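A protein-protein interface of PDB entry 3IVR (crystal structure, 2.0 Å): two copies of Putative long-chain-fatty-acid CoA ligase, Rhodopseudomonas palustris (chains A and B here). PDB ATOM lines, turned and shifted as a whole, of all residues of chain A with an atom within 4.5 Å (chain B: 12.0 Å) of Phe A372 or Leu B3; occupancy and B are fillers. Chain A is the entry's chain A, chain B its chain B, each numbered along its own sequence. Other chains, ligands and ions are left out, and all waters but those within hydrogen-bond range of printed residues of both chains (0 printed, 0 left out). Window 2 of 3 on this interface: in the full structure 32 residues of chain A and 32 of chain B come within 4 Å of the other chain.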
ATOM      1  N   LEU A 352      20.287 -12.824  13.151  1.00  0.00           N
ATOM      2  CA  LEU A 352      21.380 -12.217  13.893  1.00  0.00           C
ATOM      3  C   LEU A 352      21.017 -11.957  15.360  1.00  0.00           C
ATOM      4  O   LEU A 352      19.864 -11.679  15.683  1.00  0.00           O
ATOM      5  CB  LEU A 352      21.806 -10.912  13.206  1.00  0.00           C
ATOM      6  CG  LEU A 352      22.928 -10.085  13.843  1.00  0.00           C
ATOM      7  CD1 LEU A 352      24.237 -10.722  13.588  1.00  0.00           C
ATOM      8  CD2 LEU A 352      22.966  -8.696  13.308  1.00  0.00           C
ATOM      9  N   ARG A 353      22.026 -12.055  16.227  1.00  0.00           N
ATOM     10  CA  ARG A 353      21.948 -11.618  17.614  1.00  0.00           C
ATOM     11  C   ARG A 353      23.148 -10.760  17.939  1.00  0.00           C
ATOM     12  O   ARG A 353      24.217 -10.904  17.317  1.00  0.00           O
ATOM     13  CB  ARG A 353      21.925 -12.828  18.561  1.00  0.00           C
ATOM     14  CG  ARG A 353      20.558 -13.372  18.828  1.00  0.00           C
ATOM     15  CD  ARG A 353      20.576 -14.748  19.527  1.00  0.00           C
ATOM     16  NE  ARG A 353      19.198 -15.220  19.718  1.00  0.00           N
ATOM     17  CZ  ARG A 353      18.827 -16.458  20.059  1.00  0.00           C
ATOM     18  NH1 ARG A 353      19.720 -17.418  20.268  1.00  0.00           N
ATOM     19  NH2 ARG A 353      17.540 -16.743  20.190  1.00  0.00           N
ATOM     20  N   GLY A 354      22.981  -9.872  18.920  1.00  0.00           N
ATOM     21  CA  GLY A 354      24.094  -9.078  19.436  1.00  0.00           C
ATOM     22  C   GLY A 354      23.855  -7.574  19.364  1.00  0.00           C
ATOM     23  O   GLY A 354      22.781  -7.131  18.950  1.00  0.00           O
ATOM     24  N   VAL A 357      22.404  -5.383  16.218  1.00  0.00           N
ATOM     25  CA  VAL A 357      20.969  -5.393  15.912  1.00  0.00           C
ATOM     26  C   VAL A 357      20.357  -4.047  16.278  1.00  0.00           C
ATOM     27  O   VAL A 357      20.582  -3.517  17.366  1.00  0.00           O
ATOM     28  CB  VAL A 357      20.218  -6.554  16.594  1.00  0.00           C
ATOM     29  CG1 VAL A 357      18.737  -6.575  16.175  1.00  0.00           C
ATOM     30  CG2 VAL A 357      20.884  -7.901  16.247  1.00  0.00           C
ATOM     31  N   PHE A 358      19.622  -3.480  15.325  1.00  0.00           N
ATOM     32  CA  PHE A 358      18.955  -2.184  15.487  1.00  0.00           C
ATOM     33  C   PHE A 358      17.849  -2.167  16.565  1.00  0.00           C
ATOM     34  O   PHE A 358      17.436  -3.208  17.086  1.00  0.00           O
ATOM     35  CB  PHE A 358      18.444  -1.689  14.116  1.00  0.00           C
ATOM     36  CG  PHE A 358      17.129  -2.294  13.675  1.00  0.00           C
ATOM     37  CD1 PHE A 358      16.196  -1.505  12.999  1.00  0.00           C
ATOM     38  CD2 PHE A 358      16.820  -3.637  13.894  1.00  0.00           C
ATOM     39  CE1 PHE A 358      14.961  -2.047  12.568  1.00  0.00           C
ATOM     40  CE2 PHE A 358      15.581  -4.190  13.451  1.00  0.00           C
ATOM     41  CZ  PHE A 358      14.654  -3.380  12.800  1.00  0.00           C
ATOM     42  N   LYS A 359      17.352  -0.976  16.875  1.00  0.00           N
ATOM     43  CA  LYS A 359      16.349  -0.826  17.928  1.00  0.00           C
ATOM     44  C   LYS A 359      14.965  -1.331  17.528  1.00  0.00           C
ATOM     45  O   LYS A 359      14.206  -1.775  18.377  1.00  0.00           O
ATOM     46  CB  LYS A 359      16.286   0.624  18.404  1.00  0.00           C
ATOM     47  CG  LYS A 359      17.612   1.118  18.954  1.00  0.00           C
ATOM     48  CD  LYS A 359      17.480   2.516  19.510  1.00  0.00           C
ATOM     49  CE  LYS A 359      16.496   2.558  20.665  1.00  0.00           C
ATOM     50  NZ  LYS A 359      17.022   1.784  21.810  1.00  0.00           N
ATOM     51  N   GLY A 360      14.644  -1.281  16.239  1.00  0.00           N
ATOM     52  CA  GLY A 360      13.318  -1.694  15.764  1.00  0.00           C
ATOM     53  C   GLY A 360      12.850  -0.722  14.689  1.00  0.00           C
ATOM     54  O   GLY A 360      13.561   0.219  14.340  1.00  0.00           O
ATOM     55  N   THR A 368       8.423  -4.881  13.692  1.00  0.00           N
ATOM     56  CA  THR A 368       9.435  -5.142  14.721  1.00  0.00           C
ATOM     57  C   THR A 368       9.278  -6.508  15.395  1.00  0.00           C
ATOM     58  O   THR A 368      10.260  -7.241  15.593  1.00  0.00           O
ATOM     59  CB  THR A 368       9.379  -4.047  15.792  1.00  0.00           C
ATOM     60  OG1 THR A 368       9.642  -2.790  15.174  1.00  0.00           O
ATOM     61  CG2 THR A 368      10.395  -4.296  16.905  1.00  0.00           C
ATOM     62  N   GLN A 369       8.036  -6.830  15.742  1.00  0.00           N
ATOM     63  CA  GLN A 369       7.681  -8.085  16.382  1.00  0.00           C
ATOM     64  C   GLN A 369       7.970  -9.262  15.461  1.00  0.00           C
ATOM     65  O   GLN A 369       8.418 -10.311  15.913  1.00  0.00           O
ATOM     66  CB  GLN A 369       6.200  -8.074  16.762  1.00  0.00           C
ATOM     67  CG  GLN A 369       5.812  -9.140  17.749  1.00  0.00           C
ATOM     68  CD  GLN A 369       4.316  -9.382  17.783  1.00  0.00           C
ATOM     69  OE1 GLN A 369       3.611  -9.172  16.793  1.00  0.00           O
ATOM     70  NE2 GLN A 369       3.826  -9.839  18.926  1.00  0.00           N
ATOM     71  N   HIS A 370       7.697  -9.076  14.172  1.00  0.00           N
ATOM     72  CA  HIS A 370       8.055 -10.047  13.145  1.00  0.00           C
ATOM     73  C   HIS A 370       9.578 -10.211  13.005  1.00  0.00           C
ATOM     74  O   HIS A 370      10.080 -11.341  13.017  1.00  0.00           O
ATOM     75  CB  HIS A 370       7.427  -9.667  11.804  1.00  0.00           C
ATOM     76  CG  HIS A 370       7.553 -10.735  10.762  1.00  0.00           C
ATOM     77  ND1 HIS A 370       6.930 -11.961  10.876  1.00  0.00           N
ATOM     78  CD2 HIS A 370       8.243 -10.767   9.597  1.00  0.00           C
ATOM     79  CE1 HIS A 370       7.226 -12.700   9.822  1.00  0.00           C
ATOM     80  NE2 HIS A 370       8.022 -12.000   9.033  1.00  0.00           N
ATOM     81  N   ALA A 371      10.305  -9.089  12.947  1.00  0.00           N
ATOM     82  CA  ALA A 371      11.775  -9.103  12.818  1.00  0.00           C
ATOM     83  C   ALA A 371      12.429  -9.795  13.993  1.00  0.00           C
ATOM     84  O   ALA A 371      13.431 -10.468  13.819  1.00  0.00           O
ATOM     85  CB  ALA A 371      12.344  -7.692  12.660  1.00  0.00           C
ATOM     86  N   PHE A 372      11.839  -9.658  15.178  1.00  0.00           N
ATOM     87  CA  PHE A 372      12.494 -10.106  16.404  1.00  0.00           C
ATOM     88  C   PHE A 372      11.925 -11.407  16.956  1.00  0.00           C
ATOM     89  O   PHE A 372      12.230 -11.776  18.090  1.00  0.00           O
ATOM     90  CB  PHE A 372      12.429  -9.017  17.488  1.00  0.00           C
ATOM     91  CG  PHE A 372      13.280  -7.791  17.215  1.00  0.00           C
ATOM     92  CD1 PHE A 372      14.279  -7.794  16.243  1.00  0.00           C
ATOM     93  CD2 PHE A 372      13.101  -6.635  17.980  1.00  0.00           C
ATOM     94  CE1 PHE A 372      15.064  -6.672  16.022  1.00  0.00           C
ATOM     95  CE2 PHE A 372      13.886  -5.511  17.769  1.00  0.00           C
ATOM     96  CZ  PHE A 372      14.867  -5.528  16.779  1.00  0.00           C
ATOM     97  N   ARG A 373      11.118 -12.114  16.167  1.00  0.00           N
ATOM     98  CA  ARG A 373      10.450 -13.319  16.654  1.00  0.00           C
ATOM     99  C   ARG A 373      11.462 -14.358  17.142  1.00  0.00           C
ATOM    100  O   ARG A 373      12.557 -14.487  16.589  1.00  0.00           O
ATOM    101  CB  ARG A 373       9.476 -13.887  15.610  1.00  0.00           C
ATOM    102  CG  ARG A 373      10.117 -14.449  14.363  1.00  0.00           C
ATOM    103  CD  ARG A 373       9.098 -14.641  13.261  1.00  0.00           C
ATOM    104  NE  ARG A 373       9.687 -15.249  12.069  1.00  0.00           N
ATOM    105  CZ  ARG A 373      10.229 -14.568  11.063  1.00  0.00           C
ATOM    106  NH1 ARG A 373      10.732 -15.206  10.015  1.00  0.00           N
ATOM    107  NH2 ARG A 373      10.278 -13.248  11.094  1.00  0.00           N
ATOM    108  N   ASN A 374      11.114 -15.025  18.240  1.00  0.00           N
ATOM    109  CA  ASN A 374      11.964 -16.027  18.892  1.00  0.00           C
ATOM    110  C   ASN A 374      13.376 -15.571  19.304  1.00  0.00           C
ATOM    111  O   ASN A 374      14.289 -16.384  19.425  1.00  0.00           O
ATOM    112  CB  ASN A 374      11.988 -17.310  18.056  1.00  0.00           C
ATOM    113  CG  ASN A 374      10.598 -17.889  17.871  1.00  0.00           C
ATOM    114  OD1 ASN A 374       9.897 -18.163  18.845  1.00  0.00           O
ATOM    115  ND2 ASN A 374      10.181 -18.053  16.622  1.00  0.00           N
ATOM    116  N   GLY A 375      13.535 -14.268  19.537  1.00  0.00           N
ATOM    117  CA  GLY A 375      14.793 -13.706  20.047  1.00  0.00           C
ATOM    118  C   GLY A 375      15.965 -13.677  19.067  1.00  0.00           C
ATOM    119  O   GLY A 375      17.116 -13.644  19.485  1.00  0.00           O
ATOM    120  N   TRP A 376      15.664 -13.709  17.769  1.00  0.00           N
ATOM    121  CA  TRP A 376      16.647 -13.543  16.707  1.00  0.00           C
ATOM    122  C   TRP A 376      16.167 -12.386  15.865  1.00  0.00           C
ATOM    123  O   TRP A 376      14.970 -12.286  15.571  1.00  0.00           O
ATOM    124  CB  TRP A 376      16.664 -14.753  15.767  1.00  0.00           C
ATOM    125  CG  TRP A 376      17.406 -15.959  16.244  1.00  0.00           C
ATOM    126  CD1 TRP A 376      16.860 -17.104  16.757  1.00  0.00           C
ATOM    127  CD2 TRP A 376      18.826 -16.167  16.217  1.00  0.00           C
ATOM    128  NE1 TRP A 376      17.853 -17.999  17.071  1.00  0.00           N
ATOM    129  CE2 TRP A 376      19.067 -17.453  16.746  1.00  0.00           C
ATOM    130  CE3 TRP A 376      19.920 -15.390  15.801  1.00  0.00           C
ATOM    131  CZ2 TRP A 376      20.355 -17.981  16.870  1.00  0.00           C
ATOM    132  CZ3 TRP A 376      21.199 -15.919  15.924  1.00  0.00           C
ATOM    133  CH2 TRP A 376      21.403 -17.197  16.461  1.00  0.00           C
ATOM    134  N   HIS A 377      17.086 -11.534  15.431  1.00  0.00           N
ATOM    135  CA  HIS A 377      16.736 -10.593  14.388  1.00  0.00           C
ATOM    136  C   HIS A 377      16.692 -11.307  13.016  1.00  0.00           C
ATOM    137  O   HIS A 377      17.633 -12.004  12.637  1.00  0.00           O
ATOM    138  CB  HIS A 377      17.711  -9.427  14.326  1.00  0.00           C
ATOM    139  CG  HIS A 377      17.533  -8.602  13.097  1.00  0.00           C
ATOM    140  ND1 HIS A 377      16.365  -7.915  12.835  1.00  0.00           N
ATOM    141  CD2 HIS A 377      18.321  -8.444  12.009  1.00  0.00           C
ATOM    142  CE1 HIS A 377      16.454  -7.343  11.650  1.00  0.00           C
ATOM    143  NE2 HIS A 377      17.637  -7.639  11.134  1.00  0.00           N
ATOM    144  N   SER B   2      17.724 -10.390  25.546  1.00  0.00           N
ATOM    145  CA  SER B   2      19.154 -10.655  25.234  1.00  0.00           C
ATOM    146  C   SER B   2      19.427 -10.924  23.750  1.00  0.00           C
ATOM    147  O   SER B   2      20.539 -11.305  23.380  1.00  0.00           O
ATOM    148  CB  SER B   2      19.702 -11.801  26.083  1.00  0.00           C
ATOM    149  OG  SER B   2      19.267 -13.057  25.580  1.00  0.00           O
ATOM    150  N   LEU B   3      18.410 -10.728  22.915  1.00  0.00           N
ATOM    151  CA  LEU B   3      18.586 -10.565  21.476  1.00  0.00           C
ATOM    152  C   LEU B   3      19.766  -9.626  21.141  1.00  0.00           C
ATOM    153  O   LEU B   3      20.512  -9.875  20.203  1.00  0.00           O
ATOM    154  CB  LEU B   3      17.281 -10.042  20.878  1.00  0.00           C
ATOM    155  CG  LEU B   3      17.221  -9.174  19.626  1.00  0.00           C
ATOM    156  CD1 LEU B   3      17.365 -10.018  18.413  1.00  0.00           C
ATOM    157  CD2 LEU B   3      15.897  -8.462  19.588  1.00  0.00           C
ATOM    158  N   HIS B   4      19.948  -8.573  21.928  1.00  0.00           N
ATOM    159  CA  HIS B   4      21.055  -7.640  21.713  1.00  0.00           C
ATOM    160  C   HIS B   4      22.369  -7.965  22.452  1.00  0.00           C
ATOM    161  O   HIS B   4      23.322  -7.172  22.428  1.00  0.00           O
ATOM    162  CB  HIS B   4      20.586  -6.224  22.033  1.00  0.00           C
ATOM    163  CG  HIS B   4      19.532  -5.725  21.091  1.00  0.00           C
ATOM    164  ND1 HIS B   4      18.197  -6.048  21.217  1.00  0.00           N
ATOM    165  CD2 HIS B   4      19.623  -4.935  19.997  1.00  0.00           C
ATOM    166  CE1 HIS B   4      17.507  -5.466  20.248  1.00  0.00           C
ATOM    167  NE2 HIS B   4      18.349  -4.788  19.490  1.00  0.00           N
ATOM    168  N   ASP B   5      22.443  -9.126  23.091  1.00  0.00           N
ATOM    169  CA  ASP B   5      23.642  -9.469  23.859  1.00  0.00           C
ATOM    170  C   ASP B   5      24.640 -10.306  23.077  1.00  0.00           C
ATOM    171  O   ASP B   5      24.259 -11.192  22.286  1.00  0.00           O
ATOM    172  CB  ASP B   5      23.270 -10.181  25.161  1.00  0.00           C
ATOM    173  CG  ASP B   5      22.868  -9.214  26.259  1.00  0.00           C
ATOM    174  OD1 ASP B   5      23.737  -8.465  26.776  1.00  0.00           O
ATOM    175  OD2 ASP B   5      21.675  -9.207  26.609  1.00  0.00           O
ATOM    176  N   PHE B   6      25.915  -9.996  23.301  1.00  0.00           N
ATOM    177  CA  PHE B   6      27.055 -10.801  22.842  1.00  0.00           C
ATOM    178  C   PHE B   6      27.970 -10.954  24.056  1.00  0.00           C
ATOM    179  O   PHE B   6      28.567  -9.984  24.518  1.00  0.00           O
ATOM    180  CB  PHE B   6      27.781 -10.104  21.688  1.00  0.00           C
ATOM    181  CG  PHE B   6      28.862 -10.920  21.031  1.00  0.00           C
ATOM    182  CD1 PHE B   6      28.567 -11.735  19.953  1.00  0.00           C
ATOM    183  CD2 PHE B   6      30.184 -10.823  21.438  1.00  0.00           C
ATOM    184  CE1 PHE B   6      29.530 -12.450  19.328  1.00  0.00           C
ATOM    185  CE2 PHE B   6      31.179 -11.555  20.801  1.00  0.00           C
ATOM    186  CZ  PHE B   6      30.846 -12.376  19.730  1.00  0.00           C
ATOM    187  N   THR B   7      28.062 -12.166  24.584  1.00  0.00           N
ATOM    188  CA  THR B   7      28.810 -12.400  25.827  1.00  0.00           C
ATOM    189  C   THR B   7      30.026 -13.277  25.546  1.00  0.00           C
ATOM    190  O   THR B   7      30.276 -13.633  24.388  1.00  0.00           O
ATOM    191  CB  THR B   7      27.892 -13.057  26.872  1.00  0.00           C
ATOM    192  OG1 THR B   7      27.409 -14.312  26.369  1.00  0.00           O
ATOM    193  CG2 THR B   7      26.690 -12.145  27.186  1.00  0.00           C
ATOM    194  N   ASP B  10      29.135 -16.357  23.631  1.00  0.00           N
ATOM    195  CA  ASP B  10      29.106 -16.167  22.185  1.00  0.00           C
ATOM    196  C   ASP B  10      30.494 -16.234  21.555  1.00  0.00           C
ATOM    197  O   ASP B  10      30.621 -16.716  20.431  1.00  0.00           O
ATOM    198  CB  ASP B  10      28.384 -14.868  21.831  1.00  0.00           C
ATOM    199  CG  ASP B  10      26.963 -14.859  22.331  1.00  0.00           C
ATOM    200  OD1 ASP B  10      26.200 -15.784  21.994  1.00  0.00           O
ATOM    201  OD2 ASP B  10      26.603 -13.950  23.092  1.00  0.00           O
ATOM    202  N   ALA B 154      21.321 -22.844  28.662  1.00  0.00           N
ATOM    203  CA  ALA B 154      21.801 -21.591  29.230  1.00  0.00           C
ATOM    204  C   ALA B 154      20.683 -20.761  29.852  1.00  0.00           C
ATOM    205  O   ALA B 154      19.620 -20.626  29.255  1.00  0.00           O
ATOM    206  CB  ALA B 154      22.518 -20.790  28.162  1.00  0.00           C
ATOM    207  N   PRO B 155      20.924 -20.194  31.052  1.00  0.00           N
ATOM    208  CA  PRO B 155      19.980 -19.231  31.627  1.00  0.00           C
ATOM    209  C   PRO B 155      20.009 -17.884  30.885  1.00  0.00           C
ATOM    210  O   PRO B 155      20.907 -17.632  30.082  1.00  0.00           O
ATOM    211  CB  PRO B 155      20.486 -19.046  33.072  1.00  0.00           C
ATOM    212  CG  PRO B 155      21.585 -20.064  33.270  1.00  0.00           C
ATOM    213  CD  PRO B 155      22.092 -20.416  31.924  1.00  0.00           C
ATOM    214  N   GLU B 156      19.023 -17.034  31.153  1.00  0.00           N
ATOM    215  CA  GLU B 156      18.999 -15.681  30.614  1.00  0.00           C
ATOM    216  C   GLU B 156      19.917 -14.770  31.437  1.00  0.00           C
ATOM    217  O   GLU B 156      19.831 -14.741  32.668  1.00  0.00           O
ATOM    218  CB  GLU B 156      17.554 -15.149  30.595  1.00  0.00           C
ATOM    219  CG  GLU B 156      17.387 -13.621  30.401  1.00  0.00           C
ATOM    220  CD  GLU B 156      17.936 -13.110  29.069  1.00  0.00           C
ATOM    221  OE1 GLU B 156      17.767 -13.808  28.038  1.00  0.00           O
ATOM    222  OE2 GLU B 156      18.531 -12.004  29.061  1.00  0.00           O
ATOM    223  N   PHE B 157      20.807 -14.055  30.747  1.00  0.00           N
ATOM    224  CA  PHE B 157      21.673 -13.027  31.369  1.00  0.00           C
ATOM    225  C   PHE B 157      22.228 -12.089  30.294  1.00  0.00           C
ATOM    226  O   PHE B 157      22.259 -12.435  29.113  1.00  0.00           O
ATOM    227  CB  PHE B 157      22.823 -13.645  32.210  1.00  0.00           C
ATOM    228  CG  PHE B 157      23.833 -14.438  31.401  1.00  0.00           C
ATOM    229  CD1 PHE B 157      25.071 -13.881  31.058  1.00  0.00           C
ATOM    230  CD2 PHE B 157      23.558 -15.747  31.007  1.00  0.00           C
ATOM    231  CE1 PHE B 157      26.006 -14.609  30.310  1.00  0.00           C
ATOM    232  CE2 PHE B 157      24.486 -16.487  30.259  1.00  0.00           C
ATOM    233  CZ  PHE B 157      25.710 -15.918  29.915  1.00  0.00           C
ATOM    234  N   GLY B 158      22.683 -10.913  30.716  1.00  0.00           N
ATOM    235  CA  GLY B 158      23.234  -9.930  29.800  1.00  0.00           C
ATOM    236  C   GLY B 158      24.736  -9.803  29.899  1.00  0.00           C
ATOM    237  O   GLY B 158      25.350 -10.265  30.866  1.00  0.00           O
ATOM    238  N   ALA B 159      25.324  -9.139  28.904  1.00  0.00           N
ATOM    239  CA  ALA B 159      26.736  -8.755  28.956  1.00  0.00           C
ATOM    240  C   ALA B 159      27.039  -7.752  30.062  1.00  0.00           C
ATOM    241  O   ALA B 159      28.176  -7.684  30.537  1.00  0.00           O
ATOM    242  CB  ALA B 159      27.205  -8.227  27.596  1.00  0.00           C
ATOM    243  N   ALA B 160      26.034  -6.994  30.515  1.00  0.00           N
ATOM    244  CA  ALA B 160      26.285  -5.977  31.555  1.00  0.00           C
ATOM    245  C   ALA B 160      26.309  -6.528  32.991  1.00  0.00           C
ATOM    246  O   ALA B 160      26.695  -5.818  33.924  1.00  0.00           O
ATOM    247  CB  ALA B 160      25.295  -4.826  31.444  1.00  0.00           C
ATOM    248  N   ASP B 161      25.882  -7.773  33.154  1.00  0.00           N
ATOM    249  CA  ASP B 161      25.876  -8.459  34.452  1.00  0.00           C
ATOM    250  C   ASP B 161      27.278  -8.748  34.958  1.00  0.00           C
ATOM    251  O   ASP B 161      28.205  -8.974  34.168  1.00  0.00           O
ATOM    252  CB  ASP B 161      25.135  -9.798  34.340  1.00  0.00           C
ATOM    253  CG  ASP B 161      23.635  -9.630  34.126  1.00  0.00           C
ATOM    254  OD1 ASP B 161      23.072  -8.628  34.607  1.00  0.00           O
ATOM    255  OD2 ASP B 161      23.020 -10.505  33.481  1.00  0.00           O
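Of chain B, only Leu B3 (2.8 Å), His B4 (3.1 Å) and Asp B5 (3.6 Å) come within 4 Å of Gly A354.
No residue of chain B comes within 4 Å of Gly A360.
No residue of chain B comes within 4 Å of Ala A371.
No residue of chain B comes within 4 Å of Arg A373.
No residue of chain B comes within 4 Å of Asn A374.
Of the printed residues of chain B, Trp A376 touches Leu B3.
Of chain B, only Leu B3 comes within 4 Å of His A377.
Leu B3 touches six residues of chain A.
Of the printed residues of chain A, His B4 touches Gly A354 (3.1 Å), Val A357 (3.1 Å) and Phe A358 (3.0 Å).
Printed residues of chain A within 4 Å of Asp B5: Gly A354.
Phe B6 touches none of the printed residues of chain A.
Thr B7 touches none of the printed residues of chain A.
The nearest residue of chain B that does not touch Phe A372 is His B4 (4.4 Å).
The nearest residue of chain A that does not touch Leu B3 is Leu A352 (4.1 Å).
No position is printed for both chains.
Of the 10 pairs that touch across the chains among the printed residues, none has its exchanged pair printed and touching as well.
The backbone NH of His A377 sits at hydrogen-bond distance from the backbone carbonyl oxygen of Leu A352, 2.8 Å away.
The backbone carbonyl oxygen of Asn A374 lies within hydrogen-bond range of the guanidinium group of Arg A353, at 3.4 Å.
NE of Arg A353 lies within hydrogen-bond range of O of Gly A375.
OD1 of Asp B5 lies within hydrogen-bond range of N of Ala B159 (2.7 Å).
Arg A353 touches Leu B3.
Gly A354 touches His B4 (C to O, 3.1 Å).
Gly A354 touches Asp B5.
CG of Phe A372 touches CD2 of Leu B3, 3.6 Å away.
Leu B3 touches Gly A375.
Trp A376 touches Leu B3 (C to CD1, 3.7 Å).
N of His A377 touches CD1 of Leu B3, at 3.4 Å.
O of Leu B3 is in hydrogen-bond range of N of Gly A354.
NE2 of His B4 lies close to O of Val A357, at 3.3 Å.
O of Phe A358 sits at hydrogen-bond distance from NE2 of His B4 (3.0 Å).
Hydrophobic or aromatic side chains of chain A that line the printed part of chain B: Val A357 and Phe A372.
Printed residues of chain B that touch a printed residue of chain A: Leu B3, His B4 and Asp B5.
Hydrophobic or aromatic side chains of chain B within 4 Å of the printed part of chain A: Leu B3 and His B4.
Along chain B the printed residues that touch a printed residue of chain A span positions 3 to 5.
Among the printed residues, 10 pairs touch across the chains.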
